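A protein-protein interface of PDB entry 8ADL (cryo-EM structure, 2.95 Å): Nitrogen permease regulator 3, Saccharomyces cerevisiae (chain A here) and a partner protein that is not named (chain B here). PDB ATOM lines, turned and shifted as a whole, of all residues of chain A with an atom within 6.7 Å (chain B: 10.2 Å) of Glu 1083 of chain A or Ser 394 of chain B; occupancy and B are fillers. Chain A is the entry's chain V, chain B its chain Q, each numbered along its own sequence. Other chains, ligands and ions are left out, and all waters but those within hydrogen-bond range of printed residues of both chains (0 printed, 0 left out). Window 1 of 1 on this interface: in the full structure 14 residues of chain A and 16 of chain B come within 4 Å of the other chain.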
ATOM      1  N   VAL A 960      -8.074 -10.615  34.472  1.00  0.00           N
ATOM      2  CA  VAL A 960      -7.395 -10.903  33.213  1.00  0.00           C
ATOM      3  C   VAL A 960      -6.069 -10.151  33.187  1.00  0.00           C
ATOM      4  O   VAL A 960      -6.036  -8.937  33.420  1.00  0.00           O
ATOM      5  CB  VAL A 960      -8.271 -10.520  32.003  1.00  0.00           C
ATOM      6  CG1 VAL A 960      -7.442 -10.395  30.732  1.00  0.00           C
ATOM      7  CG2 VAL A 960      -9.384 -11.537  31.812  1.00  0.00           C
ATOM      8  N   VAL A 968      -5.644 -12.675  22.880  1.00  0.00           N
ATOM      9  CA  VAL A 968      -6.871 -12.207  22.241  1.00  0.00           C
ATOM     10  C   VAL A 968      -6.550 -11.255  21.091  1.00  0.00           C
ATOM     11  O   VAL A 968      -7.205 -11.286  20.044  1.00  0.00           O
ATOM     12  CB  VAL A 968      -7.798 -11.580  23.300  1.00  0.00           C
ATOM     13  CG1 VAL A 968      -8.886 -10.716  22.674  1.00  0.00           C
ATOM     14  CG2 VAL A 968      -8.436 -12.687  24.115  1.00  0.00           C
ATOM     15  N   THR A1071      -6.301  -6.555  34.745  1.00  0.00           N
ATOM     16  CA  THR A1071      -7.630  -5.993  34.530  1.00  0.00           C
ATOM     17  C   THR A1071      -8.642  -6.913  35.200  1.00  0.00           C
ATOM     18  O   THR A1071      -8.562  -8.135  35.058  1.00  0.00           O
ATOM     19  CB  THR A1071      -7.950  -5.845  33.027  1.00  0.00           C
ATOM     20  OG1 THR A1071      -7.111  -4.833  32.455  1.00  0.00           O
ATOM     21  CG2 THR A1071      -9.406  -5.461  32.784  1.00  0.00           C
ATOM     22  N   ILE A1073     -12.511  -7.856  35.270  1.00  0.00           N
ATOM     23  CA  ILE A1073     -13.805  -7.762  34.598  1.00  0.00           C
ATOM     24  C   ILE A1073     -14.886  -7.847  35.671  1.00  0.00           C
ATOM     25  O   ILE A1073     -15.105  -8.905  36.263  1.00  0.00           O
ATOM     26  CB  ILE A1073     -13.980  -8.858  33.542  1.00  0.00           C
ATOM     27  CG1 ILE A1073     -12.881  -8.758  32.482  1.00  0.00           C
ATOM     28  CG2 ILE A1073     -15.348  -8.752  32.892  1.00  0.00           C
ATOM     29  CD1 ILE A1073     -12.905  -9.887  31.473  1.00  0.00           C
ATOM     30  N   LEU A1074     -15.555  -6.720  35.926  1.00  0.00           N
ATOM     31  CA  LEU A1074     -16.415  -6.605  37.101  1.00  0.00           C
ATOM     32  C   LEU A1074     -17.697  -7.417  36.951  1.00  0.00           C
ATOM     33  O   LEU A1074     -18.083  -8.157  37.863  1.00  0.00           O
ATOM     34  CB  LEU A1074     -16.737  -5.135  37.367  1.00  0.00           C
ATOM     35  CG  LEU A1074     -17.087  -4.797  38.817  1.00  0.00           C
ATOM     36  CD1 LEU A1074     -15.982  -5.260  39.752  1.00  0.00           C
ATOM     37  CD2 LEU A1074     -17.334  -3.307  38.976  1.00  0.00           C
ATOM     38  N   GLU A1075     -18.371  -7.300  35.809  1.00  0.00           N
ATOM     39  CA  GLU A1075     -19.600  -8.051  35.560  1.00  0.00           C
ATOM     40  C   GLU A1075     -19.485  -8.792  34.235  1.00  0.00           C
ATOM     41  O   GLU A1075     -19.732  -8.205  33.166  1.00  0.00           O
ATOM     42  CB  GLU A1075     -20.818  -7.136  35.568  1.00  0.00           C
ATOM     43  CG  GLU A1075     -22.142  -7.879  35.473  1.00  0.00           C
ATOM     44  CD  GLU A1075     -22.505  -8.590  36.762  1.00  0.00           C
ATOM     45  OE1 GLU A1075     -22.128  -8.092  37.844  1.00  0.00           O
ATOM     46  OE2 GLU A1075     -23.167  -9.646  36.693  1.00  0.00           O
ATOM     47  N   ARG A1078     -22.506  -8.754  31.335  1.00  0.00           N
ATOM     48  CA  ARG A1078     -22.562  -7.646  30.381  1.00  0.00           C
ATOM     49  C   ARG A1078     -21.156  -7.260  29.918  1.00  0.00           C
ATOM     50  O   ARG A1078     -20.722  -6.108  29.997  1.00  0.00           O
ATOM     51  CB  ARG A1078     -23.308  -6.461  30.994  1.00  0.00           C
ATOM     52  CG  ARG A1078     -22.835  -6.041  32.381  1.00  0.00           C
ATOM     53  CD  ARG A1078     -23.671  -4.895  32.934  1.00  0.00           C
ATOM     54  NE  ARG A1078     -25.023  -5.321  33.280  1.00  0.00           N
ATOM     55  CZ  ARG A1078     -26.112  -4.983  32.604  1.00  0.00           C
ATOM     56  NH1 ARG A1078     -26.050  -4.213  31.530  1.00  0.00           N
ATOM     57  NH2 ARG A1078     -27.295  -5.431  33.016  1.00  0.00           N
ATOM     58  N   ALA A1079     -20.445  -8.250  29.391  1.00  0.00           N
ATOM     59  CA  ALA A1079     -19.120  -8.025  28.834  1.00  0.00           C
ATOM     60  C   ALA A1079     -19.208  -7.742  27.340  1.00  0.00           C
ATOM     61  O   ALA A1079     -20.145  -8.170  26.662  1.00  0.00           O
ATOM     62  CB  ALA A1079     -18.215  -9.233  29.084  1.00  0.00           C
ATOM     63  N   THR A1080     -18.216  -7.017  26.831  1.00  0.00           N
ATOM     64  CA  THR A1080     -18.172  -6.673  25.416  1.00  0.00           C
ATOM     65  C   THR A1080     -17.608  -7.857  24.630  1.00  0.00           C
ATOM     66  O   THR A1080     -17.420  -8.954  25.163  1.00  0.00           O
ATOM     67  CB  THR A1080     -17.363  -5.399  25.193  1.00  0.00           C
ATOM     68  OG1 THR A1080     -15.970  -5.679  25.365  1.00  0.00           O
ATOM     69  CG2 THR A1080     -17.790  -4.315  26.169  1.00  0.00           C
ATOM     70  N   ALA A1081     -17.334  -7.648  23.340  1.00  0.00           N
ATOM     71  CA  ALA A1081     -16.824  -8.739  22.515  1.00  0.00           C
ATOM     72  C   ALA A1081     -15.391  -9.093  22.896  1.00  0.00           C
ATOM     73  O   ALA A1081     -15.047 -10.277  23.017  1.00  0.00           O
ATOM     74  CB  ALA A1081     -16.914  -8.367  21.036  1.00  0.00           C
ATOM     75  N   ILE A1082     -14.562  -8.078  23.151  1.00  0.00           N
ATOM     76  CA  ILE A1082     -13.174  -8.338  23.511  1.00  0.00           C
ATOM     77  C   ILE A1082     -13.104  -8.908  24.923  1.00  0.00           C
ATOM     78  O   ILE A1082     -12.271  -9.775  25.210  1.00  0.00           O
ATOM     79  CB  ILE A1082     -12.324  -7.060  23.330  1.00  0.00           C
ATOM     80  CG1 ILE A1082     -10.846  -7.330  23.632  1.00  0.00           C
ATOM     81  CG2 ILE A1082     -12.868  -5.889  24.146  1.00  0.00           C
ATOM     82  CD1 ILE A1082      -9.927  -6.188  23.256  1.00  0.00           C
ATOM     83  N   GLU A1083     -14.007  -8.487  25.810  1.00  0.00           N
ATOM     84  CA  GLU A1083     -13.945  -8.973  27.181  1.00  0.00           C
ATOM     85  C   GLU A1083     -14.498 -10.387  27.277  1.00  0.00           C
ATOM     86  O   GLU A1083     -13.997 -11.195  28.066  1.00  0.00           O
ATOM     87  CB  GLU A1083     -14.703  -8.030  28.113  1.00  0.00           C
ATOM     88  CG  GLU A1083     -14.003  -6.701  28.328  1.00  0.00           C
ATOM     89  CD  GLU A1083     -14.968  -5.538  28.355  1.00  0.00           C
ATOM     90  OE1 GLU A1083     -16.158  -5.762  28.661  1.00  0.00           O
ATOM     91  OE2 GLU A1083     -14.540  -4.399  28.071  1.00  0.00           O
ATOM     92  N   LYS A1084     -15.518 -10.710  26.475  1.00  0.00           N
ATOM     93  CA  LYS A1084     -15.978 -12.092  26.410  1.00  0.00           C
ATOM     94  C   LYS A1084     -14.936 -12.983  25.751  1.00  0.00           C
ATOM     95  O   LYS A1084     -14.820 -14.164  26.105  1.00  0.00           O
ATOM     96  CB  LYS A1084     -17.311 -12.176  25.667  1.00  0.00           C
ATOM     97  CG  LYS A1084     -18.523 -12.122  26.583  1.00  0.00           C
ATOM     98  CD  LYS A1084     -19.819 -12.039  25.796  1.00  0.00           C
ATOM     99  CE  LYS A1084     -21.021 -11.981  26.726  1.00  0.00           C
ATOM    100  NZ  LYS A1084     -21.161 -10.647  27.374  1.00  0.00           N
ATOM    101  N   ARG A1085     -14.128 -12.428  24.838  1.00  0.00           N
ATOM    102  CA  ARG A1085     -12.993 -13.191  24.330  1.00  0.00           C
ATOM    103  C   ARG A1085     -11.932 -13.383  25.405  1.00  0.00           C
ATOM    104  O   ARG A1085     -11.281 -14.432  25.444  1.00  0.00           O
ATOM    105  CB  ARG A1085     -12.402 -12.511  23.096  1.00  0.00           C
ATOM    106  CG  ARG A1085     -13.214 -12.740  21.833  1.00  0.00           C
ATOM    107  CD  ARG A1085     -12.406 -12.445  20.584  1.00  0.00           C
ATOM    108  NE  ARG A1085     -13.266 -12.201  19.432  1.00  0.00           N
ATOM    109  CZ  ARG A1085     -12.948 -12.506  18.182  1.00  0.00           C
ATOM    110  NH1 ARG A1085     -11.789 -13.069  17.882  1.00  0.00           N
ATOM    111  NH2 ARG A1085     -13.813 -12.238  17.209  1.00  0.00           N
ATOM    112  N   TRP A1086     -11.772 -12.403  26.301  1.00  0.00           N
ATOM    113  CA  TRP A1086     -10.833 -12.560  27.409  1.00  0.00           C
ATOM    114  C   TRP A1086     -11.305 -13.662  28.349  1.00  0.00           C
ATOM    115  O   TRP A1086     -10.504 -14.483  28.819  1.00  0.00           O
ATOM    116  CB  TRP A1086     -10.699 -11.248  28.186  1.00  0.00           C
ATOM    117  CG  TRP A1086     -10.050 -10.118  27.450  1.00  0.00           C
ATOM    118  CD1 TRP A1086      -9.344 -10.191  26.294  1.00  0.00           C
ATOM    119  CD2 TRP A1086     -10.047  -8.737  27.833  1.00  0.00           C
ATOM    120  NE1 TRP A1086      -8.902  -8.946  25.923  1.00  0.00           N
ATOM    121  CE2 TRP A1086      -9.321  -8.034  26.854  1.00  0.00           C
ATOM    122  CE3 TRP A1086     -10.591  -8.028  28.909  1.00  0.00           C
ATOM    123  CZ2 TRP A1086      -9.124  -6.658  26.916  1.00  0.00           C
ATOM    124  CZ3 TRP A1086     -10.393  -6.660  28.969  1.00  0.00           C
ATOM    125  CH2 TRP A1086      -9.665  -5.990  27.979  1.00  0.00           C
ATOM    126  N   LEU A1087     -12.619 -13.710  28.593  1.00  0.00           N
ATOM    127  CA  LEU A1087     -13.186 -14.736  29.461  1.00  0.00           C
ATOM    128  C   LEU A1087     -13.056 -16.116  28.830  1.00  0.00           C
ATOM    129  O   LEU A1087     -12.735 -17.091  29.520  1.00  0.00           O
ATOM    130  CB  LEU A1087     -14.651 -14.424  29.764  1.00  0.00           C
ATOM    131  CG  LEU A1087     -14.969 -13.134  30.520  1.00  0.00           C
ATOM    132  CD1 LEU A1087     -16.374 -12.656  30.192  1.00  0.00           C
ATOM    133  CD2 LEU A1087     -14.808 -13.337  32.016  1.00  0.00           C
ATOM    134  N   TYR A1088     -13.298 -16.222  27.524  1.00  0.00           N
ATOM    135  CA  TYR A1088     -13.249 -17.530  26.890  1.00  0.00           C
ATOM    136  C   TYR A1088     -11.833 -17.932  26.500  1.00  0.00           C
ATOM    137  O   TYR A1088     -11.628 -19.068  26.061  1.00  0.00           O
ATOM    138  CB  TYR A1088     -14.175 -17.559  25.676  1.00  0.00           C
ATOM    139  CG  TYR A1088     -15.634 -17.588  26.067  1.00  0.00           C
ATOM    140  CD1 TYR A1088     -16.065 -18.364  27.138  1.00  0.00           C
ATOM    141  CD2 TYR A1088     -16.576 -16.831  25.384  1.00  0.00           C
ATOM    142  CE1 TYR A1088     -17.397 -18.395  27.509  1.00  0.00           C
ATOM    143  CE2 TYR A1088     -17.910 -16.855  25.750  1.00  0.00           C
ATOM    144  CZ  TYR A1088     -18.314 -17.638  26.811  1.00  0.00           C
ATOM    145  OH  TYR A1088     -19.641 -17.662  27.175  1.00  0.00           O
ATOM    146  N   ASN B 389      -5.715  -0.473  32.766  1.00  0.00           N
ATOM    147  CA  ASN B 389      -7.172  -0.565  32.730  1.00  0.00           C
ATOM    148  C   ASN B 389      -7.550  -1.457  33.909  1.00  0.00           C
ATOM    149  O   ASN B 389      -7.572  -2.682  33.798  1.00  0.00           O
ATOM    150  CB  ASN B 389      -7.669  -1.126  31.402  1.00  0.00           C
ATOM    151  CG  ASN B 389      -9.167  -0.968  31.226  1.00  0.00           C
ATOM    152  OD1 ASN B 389      -9.806  -0.184  31.927  1.00  0.00           O
ATOM    153  ND2 ASN B 389      -9.735  -1.716  30.288  1.00  0.00           N
ATOM    154  N   PHE B 390      -7.831  -0.825  35.049  1.00  0.00           N
ATOM    155  CA  PHE B 390      -8.011  -1.563  36.295  1.00  0.00           C
ATOM    156  C   PHE B 390      -9.318  -2.348  36.295  1.00  0.00           C
ATOM    157  O   PHE B 390      -9.320  -3.578  36.417  1.00  0.00           O
ATOM    158  CB  PHE B 390      -7.951  -0.598  37.479  1.00  0.00           C
ATOM    159  CG  PHE B 390      -8.230  -1.243  38.807  1.00  0.00           C
ATOM    160  CD1 PHE B 390      -7.545  -2.385  39.196  1.00  0.00           C
ATOM    161  CD2 PHE B 390      -9.162  -0.696  39.676  1.00  0.00           C
ATOM    162  CE1 PHE B 390      -7.793  -2.977  40.420  1.00  0.00           C
ATOM    163  CE2 PHE B 390      -9.413  -1.283  40.903  1.00  0.00           C
ATOM    164  CZ  PHE B 390      -8.726  -2.423  41.276  1.00  0.00           C
ATOM    165  N   VAL B 391     -10.442  -1.653  36.157  1.00  0.00           N
ATOM    166  CA  VAL B 391     -11.747  -2.297  36.164  1.00  0.00           C
ATOM    167  C   VAL B 391     -12.474  -1.937  34.873  1.00  0.00           C
ATOM    168  O   VAL B 391     -12.252  -0.876  34.279  1.00  0.00           O
ATOM    169  CB  VAL B 391     -12.557  -1.893  37.426  1.00  0.00           C
ATOM    170  CG1 VAL B 391     -12.953  -0.416  37.396  1.00  0.00           C
ATOM    171  CG2 VAL B 391     -13.768  -2.802  37.652  1.00  0.00           C
ATOM    172  N   THR B 392     -13.309  -2.864  34.411  1.00  0.00           N
ATOM    173  CA  THR B 392     -14.078  -2.663  33.192  1.00  0.00           C
ATOM    174  C   THR B 392     -15.142  -1.594  33.414  1.00  0.00           C
ATOM    175  O   THR B 392     -15.842  -1.604  34.431  1.00  0.00           O
ATOM    176  CB  THR B 392     -14.724  -3.978  32.759  1.00  0.00           C
ATOM    177  OG1 THR B 392     -13.722  -4.999  32.686  1.00  0.00           O
ATOM    178  CG2 THR B 392     -15.375  -3.829  31.399  1.00  0.00           C
ATOM    179  N   THR B 393     -15.248  -0.657  32.465  1.00  0.00           N
ATOM    180  CA  THR B 393     -16.254   0.395  32.571  1.00  0.00           C
ATOM    181  C   THR B 393     -17.664  -0.172  32.430  1.00  0.00           C
ATOM    182  O   THR B 393     -18.593   0.300  33.099  1.00  0.00           O
ATOM    183  CB  THR B 393     -15.981   1.463  31.504  1.00  0.00           C
ATOM    184  OG1 THR B 393     -14.667   1.999  31.696  1.00  0.00           O
ATOM    185  CG2 THR B 393     -16.983   2.608  31.587  1.00  0.00           C
ATOM    186  N   SER B 394     -17.832  -1.213  31.609  1.00  0.00           N
ATOM    187  CA  SER B 394     -19.145  -1.816  31.407  1.00  0.00           C
ATOM    188  C   SER B 394     -19.652  -2.541  32.648  1.00  0.00           C
ATOM    189  O   SER B 394     -20.863  -2.739  32.783  1.00  0.00           O
ATOM    190  CB  SER B 394     -19.110  -2.781  30.219  1.00  0.00           C
ATOM    191  OG  SER B 394     -18.593  -4.044  30.599  1.00  0.00           O
ATOM    192  N   GLY B 395     -18.756  -2.941  33.553  1.00  0.00           N
ATOM    193  CA  GLY B 395     -19.159  -3.545  34.808  1.00  0.00           C
ATOM    194  C   GLY B 395     -19.558  -2.576  35.899  1.00  0.00           C
ATOM    195  O   GLY B 395     -20.008  -3.015  36.961  1.00  0.00           O
ATOM    196  N   LEU B 396     -19.411  -1.275  35.667  1.00  0.00           N
ATOM    197  CA  LEU B 396     -19.779  -0.275  36.661  1.00  0.00           C
ATOM    198  C   LEU B 396     -21.244   0.122  36.519  1.00  0.00           C
ATOM    199  O   LEU B 396     -21.665   1.166  37.017  1.00  0.00           O
ATOM    200  CB  LEU B 396     -18.887   0.963  36.542  1.00  0.00           C
ATOM    201  CG  LEU B 396     -17.382   0.771  36.733  1.00  0.00           C
ATOM    202  CD1 LEU B 396     -16.634   2.044  36.376  1.00  0.00           C
ATOM    203  CD2 LEU B 396     -17.077   0.358  38.164  1.00  0.00           C
ATOM    204  N   VAL B 445     -32.351  -2.969  29.678  1.00  0.00           N
ATOM    205  CA  VAL B 445     -31.371  -2.062  30.265  1.00  0.00           C
ATOM    206  C   VAL B 445     -30.758  -1.224  29.152  1.00  0.00           C
ATOM    207  O   VAL B 445     -30.231  -1.767  28.171  1.00  0.00           O
ATOM    208  CB  VAL B 445     -30.289  -2.834  31.038  1.00  0.00           C
ATOM    209  CG1 VAL B 445     -29.274  -1.874  31.640  1.00  0.00           C
ATOM    210  CG2 VAL B 445     -30.924  -3.696  32.119  1.00  0.00           C
ATOM    211  N   PHE B 446     -30.821   0.094  29.302  1.00  0.00           N
ATOM    212  CA  PHE B 446     -30.252   1.016  28.328  1.00  0.00           C
ATOM    213  C   PHE B 446     -28.828   1.373  28.729  1.00  0.00           C
ATOM    214  O   PHE B 446     -28.577   1.764  29.874  1.00  0.00           O
ATOM    215  CB  PHE B 446     -31.110   2.275  28.217  1.00  0.00           C
ATOM    216  CG  PHE B 446     -32.351   2.090  27.395  1.00  0.00           C
ATOM    217  CD1 PHE B 446     -33.526   1.648  27.982  1.00  0.00           C
ATOM    218  CD2 PHE B 446     -32.344   2.359  26.035  1.00  0.00           C
ATOM    219  CE1 PHE B 446     -34.673   1.476  27.228  1.00  0.00           C
ATOM    220  CE2 PHE B 446     -33.488   2.190  25.274  1.00  0.00           C
ATOM    221  CZ  PHE B 446     -34.654   1.747  25.872  1.00  0.00           C
ATOM    222  N   GLU B 447     -27.897   1.237  27.786  1.00  0.00           N
ATOM    223  CA  GLU B 447     -26.503   1.578  28.034  1.00  0.00           C
ATOM    224  C   GLU B 447     -26.099   2.928  27.459  1.00  0.00           C
ATOM    225  O   GLU B 447     -25.234   3.596  28.032  1.00  0.00           O
ATOM    226  CB  GLU B 447     -25.583   0.496  27.460  1.00  0.00           C
ATOM    227  CG  GLU B 447     -25.184  -0.573  28.463  1.00  0.00           C
ATOM    228  CD  GLU B 447     -23.995  -1.392  28.001  1.00  0.00           C
ATOM    229  OE1 GLU B 447     -23.561  -1.211  26.844  1.00  0.00           O
ATOM    230  OE2 GLU B 447     -23.496  -2.216  28.796  1.00  0.00           O
ATOM    231  N   CYS B 457     -28.076   2.461  22.237  1.00  0.00           N
ATOM    232  CA  CYS B 457     -27.390   1.209  22.550  1.00  0.00           C
ATOM    233  C   CYS B 457     -28.048   0.617  23.787  1.00  0.00           C
ATOM    234  O   CYS B 457     -27.894   1.151  24.890  1.00  0.00           O
ATOM    235  CB  CYS B 457     -25.895   1.431  22.775  1.00  0.00           C
ATOM    236  SG  CYS B 457     -25.007  -0.028  23.369  1.00  0.00           S
ATOM    237  N   THR B 459     -29.271  -3.028  26.060  1.00  0.00           N
ATOM    238  CA  THR B 459     -28.941  -4.405  26.403  1.00  0.00           C
ATOM    239  C   THR B 459     -30.164  -5.107  26.979  1.00  0.00           C
ATOM    240  O   THR B 459     -30.938  -4.507  27.733  1.00  0.00           O
ATOM    241  CB  THR B 459     -27.792  -4.460  27.414  1.00  0.00           C
ATOM    242  OG1 THR B 459     -28.212  -3.872  28.650  1.00  0.00           O
ATOM    243  CG2 THR B 459     -26.585  -3.699  26.892  1.00  0.00           C
ATOM    244  N   PHE B 474     -27.714 -12.916  26.642  1.00  0.00           N
ATOM    245  CA  PHE B 474     -27.460 -11.483  26.711  1.00  0.00           C
ATOM    246  C   PHE B 474     -27.094 -10.958  25.328  1.00  0.00           C
ATOM    247  O   PHE B 474     -26.175 -11.470  24.681  1.00  0.00           O
ATOM    248  CB  PHE B 474     -26.332 -11.195  27.701  1.00  0.00           C
ATOM    249  CG  PHE B 474     -26.321  -9.786  28.221  1.00  0.00           C
ATOM    250  CD1 PHE B 474     -25.635  -8.788  27.548  1.00  0.00           C
ATOM    251  CD2 PHE B 474     -26.986  -9.465  29.393  1.00  0.00           C
ATOM    252  CE1 PHE B 474     -25.624  -7.492  28.030  1.00  0.00           C
ATOM    253  CE2 PHE B 474     -26.979  -8.173  29.880  1.00  0.00           C
ATOM    254  CZ  PHE B 474     -26.298  -7.186  29.198  1.00  0.00           C
ATOM    255  N   ARG B 476     -26.409  -7.372  22.876  1.00  0.00           N
ATOM    256  CA  ARG B 476     -26.141  -5.946  22.755  1.00  0.00           C
ATOM    257  C   ARG B 476     -26.504  -5.498  21.347  1.00  0.00           C
ATOM    258  O   ARG B 476     -25.888  -5.940  20.372  1.00  0.00           O
ATOM    259  CB  ARG B 476     -24.678  -5.627  23.058  1.00  0.00           C
ATOM    260  CG  ARG B 476     -24.370  -5.496  24.537  1.00  0.00           C
ATOM    261  CD  ARG B 476     -23.384  -4.369  24.797  1.00  0.00           C
ATOM    262  NE  ARG B 476     -23.166  -4.157  26.223  1.00  0.00           N
ATOM    263  CZ  ARG B 476     -22.239  -4.782  26.936  1.00  0.00           C
ATOM    264  NH1 ARG B 476     -21.426  -5.667  26.387  1.00  0.00           N
ATOM    265  NH2 ARG B 476     -22.129  -4.512  28.234  1.00  0.00           N
ATOM    266  N   GLU B 497     -23.837  -6.342  18.242  1.00  0.00           N
ATOM    267  CA  GLU B 497     -22.461  -6.638  18.609  1.00  0.00           C
ATOM    268  C   GLU B 497     -22.172  -8.124  18.411  1.00  0.00           C
ATOM    269  O   GLU B 497     -23.045  -8.976  18.596  1.00  0.00           O
ATOM    270  CB  GLU B 497     -22.204  -6.223  20.060  1.00  0.00           C
ATOM    271  CG  GLU B 497     -20.751  -6.291  20.496  1.00  0.00           C
ATOM    272  CD  GLU B 497     -20.490  -5.514  21.767  1.00  0.00           C
ATOM    273  OE1 GLU B 497     -21.090  -4.433  21.941  1.00  0.00           O
ATOM    274  OE2 GLU B 497     -19.678  -5.982  22.588  1.00  0.00           O
ATOM    275  N   GLU B 498     -20.939  -8.425  18.004  1.00  0.00           N
ATOM    276  CA  GLU B 498     -20.527  -9.797  17.730  1.00  0.00           C
ATOM    277  C   GLU B 498     -20.519 -10.593  19.030  1.00  0.00           C
ATOM    278  O   GLU B 498     -19.708 -10.332  19.924  1.00  0.00           O
ATOM    279  CB  GLU B 498     -19.151  -9.811  17.074  1.00  0.00           C
ATOM    280  CG  GLU B 498     -19.128  -9.246  15.664  1.00  0.00           C
ATOM    281  CD  GLU B 498     -17.809  -9.496  14.959  1.00  0.00           C
ATOM    282  OE1 GLU B 498     -16.867  -9.989  15.614  1.00  0.00           O
ATOM    283  OE2 GLU B 498     -17.714  -9.198  13.750  1.00  0.00           O
ATOM    284  N   ASN B 499     -21.420 -11.565  19.134  1.00  0.00           N
ATOM    285  CA  ASN B 499     -21.578 -12.371  20.337  1.00  0.00           C
ATOM    286  C   ASN B 499     -21.202 -13.813  20.030  1.00  0.00           C
ATOM    287  O   ASN B 499     -21.632 -14.370  19.015  1.00  0.00           O
ATOM    288  CB  ASN B 499     -23.014 -12.299  20.860  1.00  0.00           C
ATOM    289  CG  ASN B 499     -23.117 -12.641  22.334  1.00  0.00           C
ATOM    290  OD1 ASN B 499     -22.157 -13.114  22.944  1.00  0.00           O
ATOM    291  ND2 ASN B 499     -24.287 -12.403  22.916  1.00  0.00           N
ATOM    292  N   SER B 500     -20.397 -14.409  20.911  1.00  0.00           N
ATOM    293  CA  SER B 500     -20.027 -15.811  20.749  1.00  0.00           C
ATOM    294  C   SER B 500     -21.202 -16.739  21.019  1.00  0.00           C
ATOM    295  O   SER B 500     -21.280 -17.823  20.430  1.00  0.00           O
ATOM    296  CB  SER B 500     -18.862 -16.153  21.672  1.00  0.00           C
ATOM    297  OG  SER B 500     -19.238 -15.985  23.027  1.00  0.00           O
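The backbone carbonyl oxygen (O) of Val 391 of chain B lies close to the side-chain amide oxygen (OD1) of Asn 389 of chain B, 3.5 Å away.
The backbone carbonyl oxygen (O) of Phe 474 of chain B lies within hydrogen-bond range of the side-chain amide nitrogen (ND2) of Asn 499 of chain B (2.7 Å).
The side-chain carboxylate (OE1) of Glu 1083 of chain A lies within hydrogen-bond range of the backbone NH (N) of Thr 1080 of chain A (3.0 Å).
N of Glu 497 of chain B is in hydrogen-bond range of O of Arg 476 of chain B (3.0 Å).
The guanidinium group (NH2) of Arg 476 of chain B lies within salt-bridge range of the side-chain carboxylate (OE2) of Glu 447 of chain B (2.7 Å).
The backbone NH (N) of Thr 459 of chain B lies within hydrogen-bond range of the backbone carbonyl oxygen (O) of Val 445 of chain B.
Phe 390 of chain B touches Thr 1071 of chain A (O to CA, 3.5 Å).
Ile 1073 of chain A touches Thr 392 of chain B (CA to OG1, 3.4 Å).
CD2 of Leu 1074 of chain A touches O of Gly 395 of chain B, at 3.4 Å.
N of Glu 1075 of chain A touches CA of Gly 395 of chain B, at 3.97 Å.
Arg 1078 of chain A touches Val 445 of chain B (NH1 to CG1, 3.98 Å).
Arg 1078 of chain A touches Thr 459 of chain B (NH1 to OG1, 3.6 Å).
N of Thr 1080 of chain A touches NH1 of Arg 476 of chain B, 3.5 Å away.
Thr 1080 of chain A touches Glu 497 of chain B.
Ala 1081 of chain A touches Glu 498 of chain B (CB to O, 3.6 Å).
Thr 392 of chain B touches Glu 1083 of chain A.
Of chain B, only Thr 392 (3.4 Å) and Ser 394 (3.6 Å) come within 4 Å of Glu 1083 of chain A.
Ser 394 of chain B touches just these residues of chain A: Arg 1078 (3.0 Å) and Glu 1083 (3.6 Å).
Of chain B, only Arg 476 and Glu 497 come within 4 Å of Thr 1080 of chain A.
Ala 1081 of chain A touches just these residues of chain B: Glu 497 (3.0 Å) and Glu 498 (3.6 Å).
No residue of chain B comes within 4 Å of Ile 1082 of chain A.
No residue of chain B comes within 4 Å of Trp 1086 of chain A.
Of the printed residues of chain A, Asn 389 of chain B touches Thr 1071 (2.6 Å).
Printed residues of chain A within 4 Å of Glu 498 of chain B: Ala 1081.
Of the printed residues of chain B, Tyr 1088 of chain A touches Ser 500.
Glu 447 of chain B touches none of the printed residues of chain A.
The nearest residue of chain B that does not touch Glu 1083 of chain A is Arg 476 of chain B (5.7 Å).
NH2 of Arg 476 of chain B lies within hydrogen-bond range of O of Arg 1078 of chain A (2.8 Å).
The guanidinium group (NH1) of Arg 476 of chain B is in hydrogen-bond range of the backbone carbonyl oxygen (O) of Ala 1079 of chain A (2.8 Å).
The side-chain carboxylate (OE2) of Glu 497 of chain B sits at hydrogen-bond distance from the backbone NH (N) of Ala 1081 of chain A (3.0 Å).
The backbone carbonyl oxygen of Arg 1078 of chain A sits at hydrogen-bond distance from the side-chain hydroxyl of Ser 394 of chain B, at 3.0 Å.
The backbone carbonyl oxygen (O) of Asn 389 of chain B lies within hydrogen-bond range of the side-chain hydroxyl (OG1) of Thr 1071 of chain A (2.6 Å).
Of the 17 printed residues of chain A, 11 touch a printed residue of chain B.
Hydrophobic or aromatic side chains of chain A that line the printed part of chain B: Ile 1073, Leu 1074, Ala 1081 and Tyr 1088.
Among the printed residues, no Asp or Glu carboxylate lies within 4 Å of a Lys or Arg side-chain nitrogen of the other chain.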
